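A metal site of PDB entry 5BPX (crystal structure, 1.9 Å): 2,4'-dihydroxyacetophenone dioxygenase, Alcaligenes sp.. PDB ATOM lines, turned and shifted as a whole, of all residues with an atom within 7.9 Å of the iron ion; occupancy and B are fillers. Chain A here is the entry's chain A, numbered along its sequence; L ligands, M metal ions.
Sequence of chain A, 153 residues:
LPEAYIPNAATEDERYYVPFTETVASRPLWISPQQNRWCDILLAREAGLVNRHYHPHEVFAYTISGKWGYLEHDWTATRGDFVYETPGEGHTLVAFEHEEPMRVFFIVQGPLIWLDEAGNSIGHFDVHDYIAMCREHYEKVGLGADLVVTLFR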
ATOM      1  N   PHE A  20     -11.474   2.080   7.547  1.00  0.00           N
ATOM      2  CA  PHE A  20     -12.378   1.904   6.399  1.00  0.00           C
ATOM      3  C   PHE A  20     -11.958   0.654   5.632  1.00  0.00           C
ATOM      4  O   PHE A  20     -12.729  -0.266   5.441  1.00  0.00           O
ATOM      5  CB  PHE A  20     -12.241   3.162   5.539  1.00  0.00           C
ATOM      6  CG  PHE A  20     -13.061   3.145   4.309  1.00  0.00           C
ATOM      7  CD1 PHE A  20     -14.416   2.819   4.338  1.00  0.00           C
ATOM      8  CD2 PHE A  20     -12.452   3.387   3.076  1.00  0.00           C
ATOM      9  CE1 PHE A  20     -15.192   2.778   3.183  1.00  0.00           C
ATOM     10  CE2 PHE A  20     -13.250   3.387   1.883  1.00  0.00           C
ATOM     11  CZ  PHE A  20     -14.614   3.092   1.952  1.00  0.00           C
ATOM     12  N   VAL A  50      -7.797   1.138  -1.646  1.00  0.00           N
ATOM     13  CA  VAL A  50      -9.277   1.095  -1.556  1.00  0.00           C
ATOM     14  C   VAL A  50      -9.739   0.381  -2.859  1.00  0.00           C
ATOM     15  O   VAL A  50      -9.471   0.835  -3.965  1.00  0.00           O
ATOM     16  CB  VAL A  50      -9.942   2.458  -1.392  1.00  0.00           C
ATOM     17  CG1 VAL A  50     -11.465   2.299  -1.385  1.00  0.00           C
ATOM     18  CG2 VAL A  50      -9.476   3.228  -0.126  1.00  0.00           C
ATOM     19  N   ASN A  51     -10.417  -0.744  -2.725  1.00  0.00           N
ATOM     20  CA  ASN A  51     -10.891  -1.486  -3.924  1.00  0.00           C
ATOM     21  C   ASN A  51     -11.715  -0.717  -4.877  1.00  0.00           C
ATOM     22  O   ASN A  51     -12.308   0.311  -4.516  1.00  0.00           O
ATOM     23  CB  ASN A  51     -11.685  -2.699  -3.486  1.00  0.00           C
ATOM     24  CG  ASN A  51     -10.816  -3.791  -2.860  1.00  0.00           C
ATOM     25  OD1 ASN A  51      -9.602  -3.879  -3.047  1.00  0.00           O
ATOM     26  ND2 ASN A  51     -11.455  -4.626  -2.105  1.00  0.00           N
ATOM     27  N   ARG A  52     -11.679  -1.154  -6.141  1.00  0.00           N
ATOM     28  CA  ARG A  52     -12.376  -0.475  -7.169  1.00  0.00           C
ATOM     29  C   ARG A  52     -13.840  -0.210  -6.868  1.00  0.00           C
ATOM     30  O   ARG A  52     -14.543  -1.116  -6.325  1.00  0.00           O
ATOM     31  CB  ARG A  52     -12.270  -1.263  -8.473  1.00  0.00           C
ATOM     32  CG  ARG A  52     -12.691  -0.373  -9.608  1.00  0.00           C
ATOM     33  CD  ARG A  52     -12.069  -0.795 -10.899  1.00  0.00           C
ATOM     34  NE  ARG A  52     -12.498  -2.118 -11.280  1.00  0.00           N
ATOM     35  CZ  ARG A  52     -13.188  -2.383 -12.411  1.00  0.00           C
ATOM     36  NH1 ARG A  52     -13.582  -1.391 -13.216  1.00  0.00           N
ATOM     37  NH2 ARG A  52     -13.563  -3.650 -12.702  1.00  0.00           N
ATOM     38  N   HIS A  53     -14.278   0.991  -7.201  1.00  0.00           N
ATOM     39  CA  HIS A  53     -15.648   1.436  -6.967  1.00  0.00           C
ATOM     40  C   HIS A  53     -15.968   2.605  -7.846  1.00  0.00           C
ATOM     41  O   HIS A  53     -15.054   3.234  -8.413  1.00  0.00           O
ATOM     42  CB  HIS A  53     -15.878   1.786  -5.460  1.00  0.00           C
ATOM     43  CG  HIS A  53     -15.072   2.982  -5.040  1.00  0.00           C
ATOM     44  ND1 HIS A  53     -13.782   2.862  -4.563  1.00  0.00           N
ATOM     45  CD2 HIS A  53     -15.355   4.306  -5.064  1.00  0.00           C
ATOM     46  CE1 HIS A  53     -13.294   4.083  -4.357  1.00  0.00           C
ATOM     47  NE2 HIS A  53     -14.237   4.990  -4.618  1.00  0.00           N
ATOM     48  N   TYR A  54     -17.276   2.946  -8.043  1.00  0.00           N
ATOM     49  CA  TYR A  54     -17.636   4.216  -8.647  1.00  0.00           C
ATOM     50  C   TYR A  54     -18.607   4.958  -7.837  1.00  0.00           C
ATOM     51  O   TYR A  54     -19.164   4.399  -6.896  1.00  0.00           O
ATOM     52  CB  TYR A  54     -18.129   4.040 -10.098  1.00  0.00           C
ATOM     53  CG  TYR A  54     -19.597   3.563 -10.211  1.00  0.00           C
ATOM     54  CD1 TYR A  54     -19.882   2.247 -10.117  1.00  0.00           C
ATOM     55  CD2 TYR A  54     -20.632   4.491 -10.269  1.00  0.00           C
ATOM     56  CE1 TYR A  54     -21.246   1.792 -10.236  1.00  0.00           C
ATOM     57  CE2 TYR A  54     -21.956   4.083 -10.377  1.00  0.00           C
ATOM     58  CZ  TYR A  54     -22.240   2.733 -10.336  1.00  0.00           C
ATOM     59  OH  TYR A  54     -23.563   2.224 -10.426  1.00  0.00           O
ATOM     60  N   HIS A  55     -18.717   6.248  -8.108  1.00  0.00           N
ATOM     61  CA  HIS A  55     -19.590   7.134  -7.468  1.00  0.00           C
ATOM     62  C   HIS A  55     -20.590   7.569  -8.597  1.00  0.00           C
ATOM     63  O   HIS A  55     -20.182   7.941  -9.699  1.00  0.00           O
ATOM     64  CB  HIS A  55     -18.938   8.377  -6.891  1.00  0.00           C
ATOM     65  CG  HIS A  55     -17.788   8.120  -5.958  1.00  0.00           C
ATOM     66  ND1 HIS A  55     -17.883   8.297  -4.607  1.00  0.00           N
ATOM     67  CD2 HIS A  55     -16.495   7.748  -6.212  1.00  0.00           C
ATOM     68  CE1 HIS A  55     -16.703   8.002  -4.048  1.00  0.00           C
ATOM     69  NE2 HIS A  55     -15.838   7.670  -5.005  1.00  0.00           N
ATOM     70  N   HIS A  57     -22.079  10.277  -8.356  1.00  0.00           N
ATOM     71  CA  HIS A  57     -21.783  11.686  -8.405  1.00  0.00           C
ATOM     72  C   HIS A  57     -20.273  12.046  -8.219  1.00  0.00           C
ATOM     73  O   HIS A  57     -19.483  11.183  -8.201  1.00  0.00           O
ATOM     74  CB  HIS A  57     -22.580  12.386  -7.345  1.00  0.00           C
ATOM     75  CG  HIS A  57     -24.035  12.083  -7.454  1.00  0.00           C
ATOM     76  ND1 HIS A  57     -24.841  12.740  -8.362  1.00  0.00           N
ATOM     77  CD2 HIS A  57     -24.802  11.126  -6.881  1.00  0.00           C
ATOM     78  CE1 HIS A  57     -26.059  12.235  -8.290  1.00  0.00           C
ATOM     79  NE2 HIS A  57     -26.065  11.243  -7.409  1.00  0.00           N
ATOM     80  N   VAL A  59     -16.545  13.762  -6.844  1.00  0.00           N
ATOM     81  CA  VAL A  59     -15.638  13.757  -5.688  1.00  0.00           C
ATOM     82  C   VAL A  59     -14.617  14.882  -5.911  1.00  0.00           C
ATOM     83  O   VAL A  59     -14.135  15.113  -7.051  1.00  0.00           O
ATOM     84  CB  VAL A  59     -14.931  12.398  -5.602  1.00  0.00           C
ATOM     85  CG1 VAL A  59     -13.878  12.385  -4.477  1.00  0.00           C
ATOM     86  CG2 VAL A  59     -15.954  11.294  -5.355  1.00  0.00           C
ATOM     87  N   TYR A  70      -5.234   7.467  -8.298  1.00  0.00           N
ATOM     88  CA  TYR A  70      -6.111   6.412  -8.730  1.00  0.00           C
ATOM     89  C   TYR A  70      -5.419   5.703  -9.896  1.00  0.00           C
ATOM     90  O   TYR A  70      -4.802   6.330 -10.767  1.00  0.00           O
ATOM     91  CB  TYR A  70      -7.494   6.960  -9.167  1.00  0.00           C
ATOM     92  CG  TYR A  70      -8.329   7.652  -8.157  1.00  0.00           C
ATOM     93  CD1 TYR A  70      -8.991   6.955  -7.208  1.00  0.00           C
ATOM     94  CD2 TYR A  70      -8.495   9.074  -8.207  1.00  0.00           C
ATOM     95  CE1 TYR A  70      -9.839   7.613  -6.259  1.00  0.00           C
ATOM     96  CE2 TYR A  70      -9.339   9.733  -7.321  1.00  0.00           C
ATOM     97  CZ  TYR A  70      -9.972   8.982  -6.322  1.00  0.00           C
ATOM     98  OH  TYR A  70     -10.822   9.548  -5.376  1.00  0.00           O
ATOM     99  N   GLU A  85     -12.858  14.137  -9.476  1.00  0.00           N
ATOM    100  CA  GLU A  85     -13.326  12.990 -10.215  1.00  0.00           C
ATOM    101  C   GLU A  85     -14.718  13.133 -10.781  1.00  0.00           C
ATOM    102  O   GLU A  85     -15.694  13.420 -10.077  1.00  0.00           O
ATOM    103  CB  GLU A  85     -13.164  11.736  -9.350  1.00  0.00           C
ATOM    104  CG  GLU A  85     -11.839  11.128  -9.766  1.00  0.00           C
ATOM    105  CD  GLU A  85     -12.027  10.245 -11.048  1.00  0.00           C
ATOM    106  OE1 GLU A  85     -12.503  10.546 -12.248  1.00  0.00           O
ATOM    107  OE2 GLU A  85     -11.694   9.125 -10.740  1.00  0.00           O
ATOM    108  N   GLU A  89     -17.267   7.470 -12.885  1.00  0.00           N
ATOM    109  CA  GLU A  89     -15.976   6.836 -13.246  1.00  0.00           C
ATOM    110  C   GLU A  89     -15.485   5.811 -12.154  1.00  0.00           C
ATOM    111  O   GLU A  89     -15.352   6.167 -10.964  1.00  0.00           O
ATOM    112  CB  GLU A  89     -14.895   7.903 -13.519  1.00  0.00           C
ATOM    113  CG  GLU A  89     -15.102   8.628 -14.846  1.00  0.00           C
ATOM    114  CD  GLU A  89     -15.165   7.641 -16.013  1.00  0.00           C
ATOM    115  OE1 GLU A  89     -14.207   6.845 -16.196  1.00  0.00           O
ATOM    116  OE2 GLU A  89     -16.207   7.636 -16.706  1.00  0.00           O
ATOM    117  N   GLY A  90     -15.274   4.567 -12.555  1.00  0.00           N
ATOM    118  CA  GLY A  90     -14.776   3.468 -11.642  1.00  0.00           C
ATOM    119  C   GLY A  90     -13.297   3.751 -11.315  1.00  0.00           C
ATOM    120  O   GLY A  90     -12.520   4.071 -12.199  1.00  0.00           O
ATOM    121  N   HIS A  91     -12.899   3.710 -10.043  1.00  0.00           N
ATOM    122  CA  HIS A  91     -11.496   4.024  -9.719  1.00  0.00           C
ATOM    123  C   HIS A  91     -11.008   3.246  -8.486  1.00  0.00           C
ATOM    124  O   HIS A  91     -11.855   2.776  -7.660  1.00  0.00           O
ATOM    125  CB  HIS A  91     -11.281   5.494  -9.575  1.00  0.00           C
ATOM    126  CG  HIS A  91     -12.087   6.190  -8.516  1.00  0.00           C
ATOM    127  ND1 HIS A  91     -12.356   7.535  -8.587  1.00  0.00           N
ATOM    128  CD2 HIS A  91     -12.676   5.749  -7.398  1.00  0.00           C
ATOM    129  CE1 HIS A  91     -13.045   7.892  -7.502  1.00  0.00           C
ATOM    130  NE2 HIS A  91     -13.225   6.849  -6.717  1.00  0.00           N
ATOM    131  N   THR A  92      -9.689   3.020  -8.440  1.00  0.00           N
ATOM    132  CA  THR A  92      -9.029   2.244  -7.416  1.00  0.00           C
ATOM    133  C   THR A  92      -8.014   3.182  -6.763  1.00  0.00           C
ATOM    134  O   THR A  92      -7.081   3.652  -7.433  1.00  0.00           O
ATOM    135  CB  THR A  92      -8.258   1.099  -8.054  1.00  0.00           C
ATOM    136  OG1 THR A  92      -9.145   0.339  -8.938  1.00  0.00           O
ATOM    137  CG2 THR A  92      -7.707   0.171  -6.988  1.00  0.00           C
ATOM    138  N   LEU A  93      -8.250   3.567  -5.516  1.00  0.00           N
ATOM    139  CA  LEU A  93      -7.370   4.493  -4.813  1.00  0.00           C
ATOM    140  C   LEU A  93      -6.177   3.759  -4.181  1.00  0.00           C
ATOM    141  O   LEU A  93      -6.395   2.730  -3.501  1.00  0.00           O
ATOM    142  CB  LEU A  93      -8.192   5.232  -3.713  1.00  0.00           C
ATOM    143  CG  LEU A  93      -7.403   6.355  -3.045  1.00  0.00           C
ATOM    144  CD1 LEU A  93      -8.389   7.400  -2.500  1.00  0.00           C
ATOM    145  CD2 LEU A  93      -6.488   5.920  -1.851  1.00  0.00           C
ATOM    146  N   PHE A 106     -11.349  15.221   1.487  1.00  0.00           N
ATOM    147  CA  PHE A 106     -12.271  14.788   0.454  1.00  0.00           C
ATOM    148  C   PHE A 106     -13.705  15.299   0.718  1.00  0.00           C
ATOM    149  O   PHE A 106     -14.135  15.369   1.897  1.00  0.00           O
ATOM    150  CB  PHE A 106     -12.369  13.263   0.467  1.00  0.00           C
ATOM    151  CG  PHE A 106     -11.333  12.573  -0.388  1.00  0.00           C
ATOM    152  CD1 PHE A 106     -11.524  12.468  -1.749  1.00  0.00           C
ATOM    153  CD2 PHE A 106     -10.294  11.886   0.194  1.00  0.00           C
ATOM    154  CE1 PHE A 106     -10.579  11.809  -2.550  1.00  0.00           C
ATOM    155  CE2 PHE A 106      -9.355  11.198  -0.603  1.00  0.00           C
ATOM    156  CZ  PHE A 106      -9.506  11.185  -1.983  1.00  0.00           C
ATOM    157  N   VAL A 108     -17.181  14.021  -0.634  1.00  0.00           N
ATOM    158  CA  VAL A 108     -17.670  12.808  -1.337  1.00  0.00           C
ATOM    159  C   VAL A 108     -19.172  12.842  -1.465  1.00  0.00           C
ATOM    160  O   VAL A 108     -19.890  13.064  -0.508  1.00  0.00           O
ATOM    161  CB  VAL A 108     -17.293  11.550  -0.539  1.00  0.00           C
ATOM    162  CG1 VAL A 108     -17.892  10.255  -1.107  1.00  0.00           C
ATOM    163  CG2 VAL A 108     -15.772  11.452  -0.489  1.00  0.00           C
ATOM    164  N   GLN A 109     -19.677  12.605  -2.674  1.00  0.00           N
ATOM    165  CA  GLN A 109     -21.098  12.349  -2.863  1.00  0.00           C
ATOM    166  C   GLN A 109     -21.330  10.833  -3.061  1.00  0.00           C
ATOM    167  O   GLN A 109     -20.638  10.126  -3.815  1.00  0.00           O
ATOM    168  CB  GLN A 109     -21.532  13.263  -3.996  1.00  0.00           C
ATOM    169  CG  GLN A 109     -22.919  13.033  -4.461  1.00  0.00           C
ATOM    170  CD  GLN A 109     -23.935  13.362  -3.468  1.00  0.00           C
ATOM    171  OE1 GLN A 109     -24.063  14.527  -3.105  1.00  0.00           O
ATOM    172  NE2 GLN A 109     -24.756  12.334  -3.051  1.00  0.00           N
ATOM    173  N   PRO A 111     -23.751   7.181  -3.062  1.00  0.00           N
ATOM    174  CA  PRO A 111     -22.975   6.060  -2.525  1.00  0.00           C
ATOM    175  C   PRO A 111     -21.628   5.719  -3.281  1.00  0.00           C
ATOM    176  O   PRO A 111     -21.386   6.158  -4.388  1.00  0.00           O
ATOM    177  CB  PRO A 111     -23.960   4.872  -2.721  1.00  0.00           C
ATOM    178  CG  PRO A 111     -24.683   5.263  -3.979  1.00  0.00           C
ATOM    179  CD  PRO A 111     -24.926   6.739  -3.816  1.00  0.00           C
ATOM    180  N   LEU A 112     -20.741   4.953  -2.663  1.00  0.00           N
ATOM    181  CA  LEU A 112     -19.758   4.205  -3.424  1.00  0.00           C
ATOM    182  C   LEU A 112     -20.420   2.845  -3.821  1.00  0.00           C
ATOM    183  O   LEU A 112     -21.050   2.164  -2.985  1.00  0.00           O
ATOM    184  CB  LEU A 112     -18.526   3.877  -2.585  1.00  0.00           C
ATOM    185  CG  LEU A 112     -17.509   5.021  -2.280  1.00  0.00           C
ATOM    186  CD1 LEU A 112     -18.183   6.165  -1.479  1.00  0.00           C
ATOM    187  CD2 LEU A 112     -16.319   4.436  -1.518  1.00  0.00           C
ATOM    188  N   ILE A 113     -20.223   2.427  -5.064  1.00  0.00           N
ATOM    189  CA  ILE A 113     -20.609   1.095  -5.497  1.00  0.00           C
ATOM    190  C   ILE A 113     -19.365   0.324  -5.851  1.00  0.00           C
ATOM    191  O   ILE A 113     -18.603   0.765  -6.722  1.00  0.00           O
ATOM    192  CB  ILE A 113     -21.550   1.166  -6.752  1.00  0.00           C
ATOM    193  CG1 ILE A 113     -22.695   2.175  -6.515  1.00  0.00           C
ATOM    194  CG2 ILE A 113     -21.958  -0.250  -7.150  1.00  0.00           C
ATOM    195  CD1 ILE A 113     -23.700   1.794  -5.485  1.00  0.00           C
ATOM    196  N   TRP A 114     -19.151  -0.787  -5.163  1.00  0.00           N
ATOM    197  CA  TRP A 114     -17.952  -1.623  -5.261  1.00  0.00           C
ATOM    198  C   TRP A 114     -18.105  -2.428  -6.542  1.00  0.00           C
ATOM    199  O   TRP A 114     -19.261  -2.882  -6.877  1.00  0.00           O
ATOM    200  CB  TRP A 114     -17.825  -2.554  -4.076  1.00  0.00           C
ATOM    201  CG  TRP A 114     -17.756  -1.907  -2.726  1.00  0.00           C
ATOM    202  CD1 TRP A 114     -18.656  -1.991  -1.722  1.00  0.00           C
ATOM    203  CD2 TRP A 114     -16.669  -1.116  -2.225  1.00  0.00           C
ATOM    204  NE1 TRP A 114     -18.236  -1.228  -0.626  1.00  0.00           N
ATOM    205  CE2 TRP A 114     -17.023  -0.673  -0.942  1.00  0.00           C
ATOM    206  CE3 TRP A 114     -15.456  -0.698  -2.784  1.00  0.00           C
ATOM    207  CZ2 TRP A 114     -16.145   0.112  -0.170  1.00  0.00           C
ATOM    208  CZ3 TRP A 114     -14.593   0.094  -2.010  1.00  0.00           C
ATOM    209  CH2 TRP A 114     -14.948   0.478  -0.727  1.00  0.00           C
HETATM  210  C1  LIG L   1     -12.964   7.998  -2.775  1.00  0.00           C
HETATM  211  O1  LIG L   1     -12.572   7.954  -3.951  1.00  0.00           O
HETATM  212  O2  LIG L   1     -14.049   7.575  -2.375  1.00  0.00           O
HETATM  213  C2  LIG L   1     -12.144   8.740  -1.729  1.00  0.00           C
HETATM  214 FE    FE M   1     -14.003   6.919  -4.908  1.00  0.00          FE
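ND1 of His 53 sits at hydrogen-bond distance from O of Asn 51. A ring nitrogen (ND1) of His 91 is in hydrogen-bond range of the side-chain carboxylate (OE2) of Glu 85 (2.8 Å). A ring nitrogen (ND1) of His 55 lies within hydrogen-bond range of the backbone carbonyl oxygen (O) of Gln 109 (3.4 Å).
Of the 23 residues printed, 3 come within 4 Å of the iron ion. The nearest printed residue that does not touch the iron ion is Tyr 70 (4.2 Å).
The iron ion is bound by a ring nitrogen (NE2) of His 53 (2.0 Å), a ring nitrogen (NE2) of His 91 (2.0 Å), a ring nitrogen (NE2) of His 55 (2.0 Å) and an oxygen (O1) of the ligand (2.0 Å). The iron ion has four donor atoms within binding distance. Slightly farther from the iron ion lies O2 of the ligand (2.6 Å).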
